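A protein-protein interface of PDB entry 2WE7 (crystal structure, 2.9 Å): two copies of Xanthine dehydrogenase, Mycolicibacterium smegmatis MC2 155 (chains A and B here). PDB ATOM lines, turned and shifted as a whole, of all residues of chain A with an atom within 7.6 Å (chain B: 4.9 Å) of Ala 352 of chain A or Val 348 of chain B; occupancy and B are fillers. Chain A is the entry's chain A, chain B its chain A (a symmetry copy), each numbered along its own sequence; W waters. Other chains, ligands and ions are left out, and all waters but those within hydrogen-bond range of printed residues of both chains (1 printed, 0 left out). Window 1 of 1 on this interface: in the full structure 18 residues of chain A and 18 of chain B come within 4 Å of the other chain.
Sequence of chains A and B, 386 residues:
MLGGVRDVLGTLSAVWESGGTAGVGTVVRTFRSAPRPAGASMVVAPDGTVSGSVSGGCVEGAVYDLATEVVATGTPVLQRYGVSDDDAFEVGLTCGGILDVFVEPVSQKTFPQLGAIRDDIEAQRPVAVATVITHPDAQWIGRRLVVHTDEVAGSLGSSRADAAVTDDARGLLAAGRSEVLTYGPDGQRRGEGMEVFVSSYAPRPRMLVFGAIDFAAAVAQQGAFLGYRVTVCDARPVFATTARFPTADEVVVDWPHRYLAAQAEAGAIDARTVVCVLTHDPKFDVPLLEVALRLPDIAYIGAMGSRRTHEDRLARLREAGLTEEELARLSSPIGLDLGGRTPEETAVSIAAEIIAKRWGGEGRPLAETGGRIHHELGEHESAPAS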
ATOM      1  N   GLN A 222      -0.596   6.684  -1.485  1.00  0.00           N
ATOM      2  CA  GLN A 222      -0.285   6.487  -2.902  1.00  0.00           C
ATOM      3  C   GLN A 222      -1.448   6.962  -3.780  1.00  0.00           C
ATOM      4  O   GLN A 222      -1.242   7.633  -4.808  1.00  0.00           O
ATOM      5  CB  GLN A 222       0.068   5.028  -3.194  1.00  0.00           C
ATOM      6  CG  GLN A 222       1.395   4.607  -2.606  1.00  0.00           C
ATOM      7  CD  GLN A 222       2.578   5.425  -3.148  1.00  0.00           C
ATOM      8  OE1 GLN A 222       2.643   5.734  -4.330  1.00  0.00           O
ATOM      9  NE2 GLN A 222       3.522   5.755  -2.275  1.00  0.00           N
ATOM     10  N   PHE A 225      -1.409  10.657  -3.634  1.00  0.00           N
ATOM     11  CA  PHE A 225      -0.282  11.089  -4.429  1.00  0.00           C
ATOM     12  C   PHE A 225      -0.612  11.051  -5.937  1.00  0.00           C
ATOM     13  O   PHE A 225      -0.229  11.951  -6.664  1.00  0.00           O
ATOM     14  CB  PHE A 225       0.967  10.280  -4.054  1.00  0.00           C
ATOM     15  CG  PHE A 225       2.215  10.709  -4.773  1.00  0.00           C
ATOM     16  CD1 PHE A 225       3.049  11.683  -4.226  1.00  0.00           C
ATOM     17  CD2 PHE A 225       2.575  10.126  -5.995  1.00  0.00           C
ATOM     18  CE1 PHE A 225       4.217  12.072  -4.876  1.00  0.00           C
ATOM     19  CE2 PHE A 225       3.729  10.516  -6.662  1.00  0.00           C
ATOM     20  CZ  PHE A 225       4.552  11.488  -6.098  1.00  0.00           C
ATOM     21  N   LEU A 226      -1.351  10.040  -6.391  1.00  0.00           N
ATOM     22  CA  LEU A 226      -1.750   9.940  -7.802  1.00  0.00           C
ATOM     23  C   LEU A 226      -2.968  10.786  -8.183  1.00  0.00           C
ATOM     24  O   LEU A 226      -3.405  10.767  -9.338  1.00  0.00           O
ATOM     25  CB  LEU A 226      -2.044   8.492  -8.159  1.00  0.00           C
ATOM     26  CG  LEU A 226      -0.813   7.589  -8.274  1.00  0.00           C
ATOM     27  CD1 LEU A 226      -1.174   6.130  -8.030  1.00  0.00           C
ATOM     28  CD2 LEU A 226      -0.161   7.765  -9.632  1.00  0.00           C
ATOM     29  N   TYR A 300     -10.002  -0.998 -12.141  1.00  0.00           N
ATOM     30  CA  TYR A 300      -9.122  -1.882 -11.404  1.00  0.00           C
ATOM     31  C   TYR A 300      -9.795  -2.449 -10.171  1.00  0.00           C
ATOM     32  O   TYR A 300     -10.444  -1.729  -9.428  1.00  0.00           O
ATOM     33  CB  TYR A 300      -7.878  -1.107 -11.026  1.00  0.00           C
ATOM     34  CG  TYR A 300      -6.806  -1.889 -10.315  1.00  0.00           C
ATOM     35  CD1 TYR A 300      -5.845  -2.635 -11.033  1.00  0.00           C
ATOM     36  CD2 TYR A 300      -6.713  -1.849  -8.929  1.00  0.00           C
ATOM     37  CE1 TYR A 300      -4.844  -3.336 -10.374  1.00  0.00           C
ATOM     38  CE2 TYR A 300      -5.720  -2.552  -8.255  1.00  0.00           C
ATOM     39  CZ  TYR A 300      -4.794  -3.277  -8.982  1.00  0.00           C
ATOM     40  OH  TYR A 300      -3.832  -3.946  -8.282  1.00  0.00           O
ATOM     41  N   GLY A 335      -0.842  -5.820  -6.802  1.00  0.00           N
ATOM     42  CA  GLY A 335       0.434  -5.173  -7.044  1.00  0.00           C
ATOM     43  C   GLY A 335       1.208  -5.846  -8.142  1.00  0.00           C
ATOM     44  O   GLY A 335       0.952  -6.985  -8.455  1.00  0.00           O
ATOM     45  N   LEU A 336       2.210  -5.165  -8.648  1.00  0.00           N
ATOM     46  CA  LEU A 336       3.148  -5.737  -9.550  1.00  0.00           C
ATOM     47  C   LEU A 336       4.049  -6.518  -8.658  1.00  0.00           C
ATOM     48  O   LEU A 336       4.123  -6.254  -7.491  1.00  0.00           O
ATOM     49  CB  LEU A 336       3.935  -4.669 -10.251  1.00  0.00           C
ATOM     50  CG  LEU A 336       3.197  -3.837 -11.260  1.00  0.00           C
ATOM     51  CD1 LEU A 336       4.125  -2.922 -11.893  1.00  0.00           C
ATOM     52  CD2 LEU A 336       2.611  -4.670 -12.268  1.00  0.00           C
ATOM     53  N   LEU A 338       7.271  -6.922  -7.560  1.00  0.00           N
ATOM     54  CA  LEU A 338       8.566  -6.326  -7.474  1.00  0.00           C
ATOM     55  C   LEU A 338       9.409  -6.899  -6.386  1.00  0.00           C
ATOM     56  O   LEU A 338      10.483  -6.444  -6.180  1.00  0.00           O
ATOM     57  CB  LEU A 338       8.393  -4.864  -7.163  1.00  0.00           C
ATOM     58  CG  LEU A 338       7.960  -3.834  -8.182  1.00  0.00           C
ATOM     59  CD1 LEU A 338       7.489  -4.400  -9.433  1.00  0.00           C
ATOM     60  CD2 LEU A 338       6.999  -2.907  -7.594  1.00  0.00           C
ATOM     61  N   THR A 346       4.844  -2.573  -0.719  1.00  0.00           N
ATOM     62  CA  THR A 346       3.677  -3.237  -1.255  1.00  0.00           C
ATOM     63  C   THR A 346       2.780  -2.148  -1.802  1.00  0.00           C
ATOM     64  O   THR A 346       2.217  -2.271  -2.888  1.00  0.00           O
ATOM     65  CB  THR A 346       2.937  -4.016  -0.171  1.00  0.00           C
ATOM     66  OG1 THR A 346       3.890  -4.721   0.635  1.00  0.00           O
ATOM     67  CG2 THR A 346       1.960  -4.985  -0.779  1.00  0.00           C
ATOM     68  N   ALA A 347       2.677  -1.056  -1.061  1.00  0.00           N
ATOM     69  CA  ALA A 347       1.791   0.014  -1.467  1.00  0.00           C
ATOM     70  C   ALA A 347       2.225   0.607  -2.809  1.00  0.00           C
ATOM     71  O   ALA A 347       1.384   0.871  -3.667  1.00  0.00           O
ATOM     72  CB  ALA A 347       1.693   1.078  -0.385  1.00  0.00           C
ATOM     73  N   VAL A 348       3.534   0.770  -3.001  1.00  0.00           N
ATOM     74  CA  VAL A 348       4.064   1.285  -4.266  1.00  0.00           C
ATOM     75  C   VAL A 348       3.837   0.257  -5.349  1.00  0.00           C
ATOM     76  O   VAL A 348       3.440   0.595  -6.465  1.00  0.00           O
ATOM     77  CB  VAL A 348       5.556   1.640  -4.194  1.00  0.00           C
ATOM     78  CG1 VAL A 348       6.168   1.601  -5.572  1.00  0.00           C
ATOM     79  CG2 VAL A 348       5.735   2.999  -3.582  1.00  0.00           C
ATOM     80  N   SER A 349       4.042  -1.008  -5.020  1.00  0.00           N
ATOM     81  CA  SER A 349       3.784  -2.035  -6.010  1.00  0.00           C
ATOM     82  C   SER A 349       2.307  -2.051  -6.466  1.00  0.00           C
ATOM     83  O   SER A 349       2.007  -2.363  -7.609  1.00  0.00           O
ATOM     84  CB  SER A 349       4.252  -3.390  -5.514  1.00  0.00           C
ATOM     85  OG  SER A 349       3.170  -4.059  -4.921  1.00  0.00           O
ATOM     86  N   ILE A 350       1.393  -1.677  -5.586  1.00  0.00           N
ATOM     87  CA  ILE A 350       0.000  -1.527  -5.984  1.00  0.00           C
ATOM     88  C   ILE A 350      -0.181  -0.329  -6.943  1.00  0.00           C
ATOM     89  O   ILE A 350      -0.666  -0.498  -8.079  1.00  0.00           O
ATOM     90  CB  ILE A 350      -0.923  -1.402  -4.751  1.00  0.00           C
ATOM     91  CG1 ILE A 350      -0.955  -2.732  -3.999  1.00  0.00           C
ATOM     92  CG2 ILE A 350      -2.326  -1.008  -5.159  1.00  0.00           C
ATOM     93  CD1 ILE A 350      -1.581  -2.644  -2.623  1.00  0.00           C
ATOM     94  N   ALA A 351       0.222   0.864  -6.493  1.00  0.00           N
ATOM     95  CA  ALA A 351       0.174   2.073  -7.328  1.00  0.00           C
ATOM     96  C   ALA A 351       0.754   1.827  -8.711  1.00  0.00           C
ATOM     97  O   ALA A 351       0.165   2.206  -9.706  1.00  0.00           O
ATOM     98  CB  ALA A 351       0.905   3.202  -6.670  1.00  0.00           C
ATOM     99  N   ALA A 352       1.916   1.181  -8.761  1.00  0.00           N
ATOM    100  CA  ALA A 352       2.545   0.817 -10.024  1.00  0.00           C
ATOM    101  C   ALA A 352       1.604  -0.032 -10.873  1.00  0.00           C
ATOM    102  O   ALA A 352       1.392   0.291 -12.035  1.00  0.00           O
ATOM    103  CB  ALA A 352       3.844   0.099  -9.775  1.00  0.00           C
ATOM    104  N   GLU A 353       1.022  -1.086 -10.288  1.00  0.00           N
ATOM    105  CA  GLU A 353       0.044  -1.914 -11.003  1.00  0.00           C
ATOM    106  C   GLU A 353      -1.160  -1.128 -11.538  1.00  0.00           C
ATOM    107  O   GLU A 353      -1.505  -1.293 -12.705  1.00  0.00           O
ATOM    108  CB  GLU A 353      -0.424  -3.110 -10.183  1.00  0.00           C
ATOM    109  CG  GLU A 353      -1.058  -4.218 -11.045  1.00  0.00           C
ATOM    110  CD  GLU A 353      -1.622  -5.408 -10.221  1.00  0.00           C
ATOM    111  OE1 GLU A 353      -2.116  -5.205  -9.089  1.00  0.00           O
ATOM    112  OE2 GLU A 353      -1.596  -6.562 -10.724  1.00  0.00           O
ATOM    113  N   ILE A 354      -1.767  -0.264 -10.719  1.00  0.00           N
ATOM    114  CA  ILE A 354      -2.844   0.628 -11.210  1.00  0.00           C
ATOM    115  C   ILE A 354      -2.446   1.415 -12.459  1.00  0.00           C
ATOM    116  O   ILE A 354      -3.153   1.372 -13.471  1.00  0.00           O
ATOM    117  CB  ILE A 354      -3.371   1.611 -10.126  1.00  0.00           C
ATOM    118  CG1 ILE A 354      -4.224   0.849  -9.119  1.00  0.00           C
ATOM    119  CG2 ILE A 354      -4.220   2.705 -10.751  1.00  0.00           C
ATOM    120  CD1 ILE A 354      -4.193   1.416  -7.749  1.00  0.00           C
ATOM    121  N   ILE A 355      -1.328   2.133 -12.390  1.00  0.00           N
ATOM    122  CA  ILE A 355      -0.851   2.919 -13.512  1.00  0.00           C
ATOM    123  C   ILE A 355      -0.669   2.042 -14.748  1.00  0.00           C
ATOM    124  O   ILE A 355      -1.128   2.399 -15.833  1.00  0.00           O
ATOM    125  CB  ILE A 355       0.479   3.604 -13.170  1.00  0.00           C
ATOM    126  CG1 ILE A 355       0.255   4.673 -12.089  1.00  0.00           C
ATOM    127  CG2 ILE A 355       1.147   4.185 -14.412  1.00  0.00           C
ATOM    128  CD1 ILE A 355       1.544   5.155 -11.465  1.00  0.00           C
ATOM    129  N   ALA A 356      -0.021   0.891 -14.566  1.00  0.00           N
ATOM    130  CA  ALA A 356       0.306  -0.016 -15.659  1.00  0.00           C
ATOM    131  C   ALA A 356      -0.936  -0.498 -16.400  1.00  0.00           C
ATOM    132  O   ALA A 356      -0.995  -0.489 -17.636  1.00  0.00           O
ATOM    133  CB  ALA A 356       1.074  -1.200 -15.117  1.00  0.00           C
ATOM    134  N   LYS A 357      -1.934  -0.908 -15.626  1.00  0.00           N
ATOM    135  CA  LYS A 357      -3.161  -1.441 -16.180  1.00  0.00           C
ATOM    136  C   LYS A 357      -4.051  -0.390 -16.884  1.00  0.00           C
ATOM    137  O   LYS A 357      -4.984  -0.751 -17.586  1.00  0.00           O
ATOM    138  CB  LYS A 357      -3.920  -2.196 -15.101  1.00  0.00           C
ATOM    139  CG  LYS A 357      -4.657  -3.407 -15.599  1.00  0.00           C
ATOM    140  CD  LYS A 357      -5.923  -3.621 -14.770  1.00  0.00           C
ATOM    141  CE  LYS A 357      -7.054  -4.294 -15.555  1.00  0.00           C
ATOM    142  NZ  LYS A 357      -8.343  -4.261 -14.790  1.00  0.00           N
ATOM    143  N   ARG A 358      -3.779   0.900 -16.717  1.00  0.00           N
ATOM    144  CA  ARG A 358      -4.488   1.902 -17.513  1.00  0.00           C
ATOM    145  C   ARG A 358      -3.614   2.502 -18.621  1.00  0.00           C
ATOM    146  O   ARG A 358      -4.145   3.059 -19.580  1.00  0.00           O
ATOM    147  CB  ARG A 358      -5.067   3.023 -16.628  1.00  0.00           C
ATOM    148  CG  ARG A 358      -4.171   4.276 -16.446  1.00  0.00           C
ATOM    149  CD  ARG A 358      -4.859   5.395 -15.626  1.00  0.00           C
ATOM    150  NE  ARG A 358      -3.900   6.372 -15.083  1.00  0.00           N
ATOM    151  CZ  ARG A 358      -3.542   6.487 -13.796  1.00  0.00           C
ATOM    152  NH1 ARG A 358      -4.054   5.704 -12.857  1.00  0.00           N
ATOM    153  NH2 ARG A 358      -2.659   7.407 -13.436  1.00  0.00           N
ATOM    154  N   GLN B 222       8.393  10.068  -2.882  1.00  0.00           N
ATOM    155  CA  GLN B 222       8.466   8.610  -2.997  1.00  0.00           C
ATOM    156  C   GLN B 222       9.645   8.064  -2.184  1.00  0.00           C
ATOM    157  O   GLN B 222       9.519   7.050  -1.474  1.00  0.00           O
ATOM    158  CB  GLN B 222       8.554   8.173  -4.459  1.00  0.00           C
ATOM    159  CG  GLN B 222       7.273   8.399  -5.227  1.00  0.00           C
ATOM    160  CD  GLN B 222       6.079   7.626  -4.645  1.00  0.00           C
ATOM    161  OE1 GLN B 222       6.209   6.478  -4.239  1.00  0.00           O
ATOM    162  NE2 GLN B 222       4.912   8.256  -4.628  1.00  0.00           N
ATOM    163  N   LEU B 338       5.650   1.633 -17.209  1.00  0.00           N
ATOM    164  CA  LEU B 338       4.264   1.429 -16.932  1.00  0.00           C
ATOM    165  C   LEU B 338       3.363   2.251 -17.790  1.00  0.00           C
ATOM    166  O   LEU B 338       2.193   2.210 -17.612  1.00  0.00           O
ATOM    167  CB  LEU B 338       4.002   1.841 -15.509  1.00  0.00           C
ATOM    168  CG  LEU B 338       4.389   1.006 -14.308  1.00  0.00           C
ATOM    169  CD1 LEU B 338       5.253  -0.117 -14.622  1.00  0.00           C
ATOM    170  CD2 LEU B 338       4.938   1.853 -13.255  1.00  0.00           C
ATOM    171  N   GLU B 344       3.732  12.505 -11.347  1.00  0.00           N
ATOM    172  CA  GLU B 344       3.479  11.598 -10.228  1.00  0.00           C
ATOM    173  C   GLU B 344       3.583  10.131 -10.638  1.00  0.00           C
ATOM    174  O   GLU B 344       4.138   9.315  -9.912  1.00  0.00           O
ATOM    175  CB  GLU B 344       2.120  11.867  -9.583  1.00  0.00           C
ATOM    176  CG  GLU B 344       2.049  13.156  -8.739  1.00  0.00           C
ATOM    177  CD  GLU B 344       1.814  14.439  -9.564  1.00  0.00           C
ATOM    178  OE1 GLU B 344       1.724  14.376 -10.825  1.00  0.00           O
ATOM    179  OE2 GLU B 344       1.729  15.523  -8.930  1.00  0.00           O
ATOM    180  N   GLU B 345       3.112   9.821 -11.813  1.00  0.00           N
ATOM    181  CA  GLU B 345       3.182   8.494 -12.326  1.00  0.00           C
ATOM    182  C   GLU B 345       4.549   8.102 -12.729  1.00  0.00           C
ATOM    183  O   GLU B 345       4.881   6.962 -12.701  1.00  0.00           O
ATOM    184  CB  GLU B 345       2.306   8.389 -13.534  1.00  0.00           C
ATOM    185  CG  GLU B 345       0.881   8.438 -13.213  1.00  0.00           C
ATOM    186  CD  GLU B 345       0.036   8.552 -14.420  1.00  0.00           C
ATOM    187  OE1 GLU B 345      -0.352   7.518 -14.955  1.00  0.00           O
ATOM    188  OE2 GLU B 345      -0.227   9.670 -14.858  1.00  0.00           O
ATOM    189  N   THR B 346       5.340   9.054 -13.155  1.00  0.00           N
ATOM    190  CA  THR B 346       6.724   8.788 -13.480  1.00  0.00           C
ATOM    191  C   THR B 346       7.428   8.527 -12.167  1.00  0.00           C
ATOM    192  O   THR B 346       8.234   7.606 -12.046  1.00  0.00           O
ATOM    193  CB  THR B 346       7.367   9.982 -14.180  1.00  0.00           C
ATOM    194  OG1 THR B 346       6.458  10.498 -15.161  1.00  0.00           O
ATOM    195  CG2 THR B 346       8.662   9.586 -14.836  1.00  0.00           C
ATOM    196  N   ALA B 347       7.092   9.321 -11.162  1.00  0.00           N
ATOM    197  CA  ALA B 347       7.760   9.193  -9.883  1.00  0.00           C
ATOM    198  C   ALA B 347       7.508   7.815  -9.269  1.00  0.00           C
ATOM    199  O   ALA B 347       8.431   7.200  -8.735  1.00  0.00           O
ATOM    200  CB  ALA B 347       7.350  10.315  -8.942  1.00  0.00           C
ATOM    201  N   VAL B 348       6.277   7.317  -9.386  1.00  0.00           N
ATOM    202  CA  VAL B 348       5.937   5.988  -8.876  1.00  0.00           C
ATOM    203  C   VAL B 348       6.645   4.946  -9.709  1.00  0.00           C
ATOM    204  O   VAL B 348       7.188   3.977  -9.177  1.00  0.00           O
ATOM    205  CB  VAL B 348       4.427   5.710  -8.875  1.00  0.00           C
ATOM    206  CG1 VAL B 348       4.169   4.224  -8.908  1.00  0.00           C
ATOM    207  CG2 VAL B 348       3.789   6.324  -7.662  1.00  0.00           C
ATOM    208  N   SER B 349       6.685   5.155 -11.014  1.00  0.00           N
ATOM    209  CA  SER B 349       7.401   4.211 -11.849  1.00  0.00           C
ATOM    210  C   SER B 349       8.902   4.129 -11.485  1.00  0.00           C
ATOM    211  O   SER B 349       9.518   3.079 -11.601  1.00  0.00           O
ATOM    212  CB  SER B 349       7.178   4.515 -13.318  1.00  0.00           C
ATOM    213  OG  SER B 349       8.228   5.322 -13.784  1.00  0.00           O
ATOM    214  N   ILE B 350       9.474   5.221 -11.007  1.00  0.00           N
ATOM    215  CA  ILE B 350      10.842   5.181 -10.507  1.00  0.00           C
ATOM    216  C   ILE B 350      10.937   4.352  -9.207  1.00  0.00           C
ATOM    217  O   ILE B 350      11.691   3.362  -9.143  1.00  0.00           O
ATOM    218  CB  ILE B 350      11.404   6.605 -10.305  1.00  0.00           C
ATOM    219  CG1 ILE B 350      11.589   7.280 -11.664  1.00  0.00           C
ATOM    220  CG2 ILE B 350      12.724   6.570  -9.565  1.00  0.00           C
ATOM    221  CD1 ILE B 350      11.848   8.770 -11.579  1.00  0.00           C
ATOM    222  N   ALA B 351      10.165   4.745  -8.188  1.00  0.00           N
ATOM    223  CA  ALA B 351      10.105   4.004  -6.920  1.00  0.00           C
ATOM    224  C   ALA B 351       9.929   2.512  -7.147  1.00  0.00           C
ATOM    225  O   ALA B 351      10.616   1.708  -6.543  1.00  0.00           O
ATOM    226  CB  ALA B 351       8.992   4.516  -6.059  1.00  0.00           C
ATOM    227  N   ALA B 352       9.001   2.151  -8.029  1.00  0.00           N
ATOM    228  CA  ALA B 352       8.781   0.756  -8.392  1.00  0.00           C
ATOM    229  C   ALA B 352      10.066   0.124  -8.915  1.00  0.00           C
ATOM    230  O   ALA B 352      10.449  -0.935  -8.435  1.00  0.00           O
ATOM    231  CB  ALA B 352       7.674   0.649  -9.407  1.00  0.00           C
ATOM    232  N   GLU B 353      10.740   0.783  -9.866  1.00  0.00           N
ATOM    233  CA  GLU B 353      12.026   0.290 -10.374  1.00  0.00           C
ATOM    234  C   GLU B 353      13.091   0.101  -9.286  1.00  0.00           C
ATOM    235  O   GLU B 353      13.719  -0.953  -9.248  1.00  0.00           O
ATOM    236  CB  GLU B 353      12.574   1.142 -11.512  1.00  0.00           C
ATOM    237  CG  GLU B 353      13.635   0.410 -12.354  1.00  0.00           C
ATOM    238  CD  GLU B 353      14.271   1.290 -13.464  1.00  0.00           C
ATOM    239  OE1 GLU B 353      14.433   2.516 -13.273  1.00  0.00           O
ATOM    240  OE2 GLU B 353      14.640   0.743 -14.536  1.00  0.00           O
HETATM  241  O   HOH W   1       0.598  14.683  -5.810  1.00  0.00           O
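OE1 of Glu 345 of chain B lies within salt-bridge range of NH2 of Arg 358 of chain A (2.8 Å).
The side-chain amide nitrogen (NE2) of Gln 222 of chain B lies within hydrogen-bond range of the side-chain amide oxygen (OE1) of Gln 222 of chain A, 3.4 Å away.
Among the printed residues, pairs that only touch across the chains: Gln 222 of chain A with Val 348 of chain B (3.6 Å), Phe 225 of chain A with Gln 222 of chain B (3.3 Å), Phe 225 of chain A with Glu 344 of chain B (3.3 Å), Leu 226 of chain A with Glu 345 of chain B (3.8 Å), Leu 338 of chain A with Ala 352 of chain B (3.8 Å), Val 348 of chain A with Gln 222 of chain B (3.6 Å), Val 348 of chain A with Ala 352 of chain B (3.8 Å), Ala 352 of chain A with Leu 338 of chain B (3.8 Å), Ala 352 of chain A with Val 348 of chain B (3.8 Å), Ala 352 of chain A with Ala 352 of chain B (3.9 Å), Ile 355 of chain A with Leu 338 of chain B (3.8 Å), Ile 355 of chain A with Glu 345 of chain B (3.7 Å), Ile 355 of chain A with Val 348 of chain B (3.8 Å) and Ala 356 of chain A with Leu 338 of chain B (3.5 Å).
Of the printed residues of chain B, Gln 222 of chain A touches Gln 222 and Val 348.
Printed residues of chain B within 4 Å of Leu 226 of chain A: Glu 345 (3.8 Å).
Printed residues of chain B within 4 Å of Leu 338 of chain A: Ala 352 (3.8 Å).
Of the printed residues of chain B, Val 348 of chain A touches Gln 222 (3.6 Å) and Ala 352 (3.8 Å).
Ile 350 of chain A touches none of the printed residues of chain B.
Ala 352 of chain A touches just these residues of chain B: Leu 338 (3.8 Å), Val 348 (3.8 Å) and Ala 352 (3.9 Å).
No residue of chain A comes within 4 Å of Ala 347 of chain B.
Of chain A, only Gln 222 (3.6 Å), Ala 352 (3.8 Å) and Ile 355 (3.8 Å) come within 4 Å of Val 348 of chain B.
Ile 350 of chain B touches none of the printed residues of chain A.
Of the printed residues of chain A, Ala 352 of chain B touches Leu 338 (3.8 Å), Val 348 (3.8 Å) and Ala 352 (3.9 Å).
The nearest printed residue of chain B that does not touch Ala 352 of chain A is Ser 349 of chain B (5.8 Å).
The nearest printed residue of chain B that does not touch Gln 222 of chain A is Ala 351 of chain B (6.7 Å).
Of the 12 printed residues of chain B, 6 touch a printed residue of chain A.
Printed residues of chain B that touch a printed residue of chain A: Gln 222, Leu 338, Glu 344, Glu 345, Val 348 and Ala 352.
Hydrophobic or aromatic side chains of chain B within 4 Å of the printed part of chain A: Leu 338, Val 348 and Ala 352.
Of the 20 printed residues of chain A, 9 touch a printed residue of chain B.
Hydrophobic or aromatic side chains of chain A that line the printed part of chain B: Phe 225, Leu 226, Leu 338, Val 348, Ala 352 and Ile 355.
Gln 222 of chain B touches its own counterpart, Gln 222 of chain A.
Gln 222 of chain A touches Val 348 of chain B, and with the chains exchanged Val 348 of chain A touches Gln 222 of chain B.
Leu 338 of chain A touches Ala 352 of chain B, and with the chains exchanged Ala 352 of chain A touches Leu 338 of chain B.
Ala 352 of chain B touches its own counterpart, Ala 352 of chain A.
Of the 16 pairs that touch across the chains among the printed residues, 8 have their exchanged pair printed and touching as well.
Water W1 bridges O of Phe 225 of chain A (3.0 Å) and OE2 of Glu 344 of chain B (3.4 Å).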
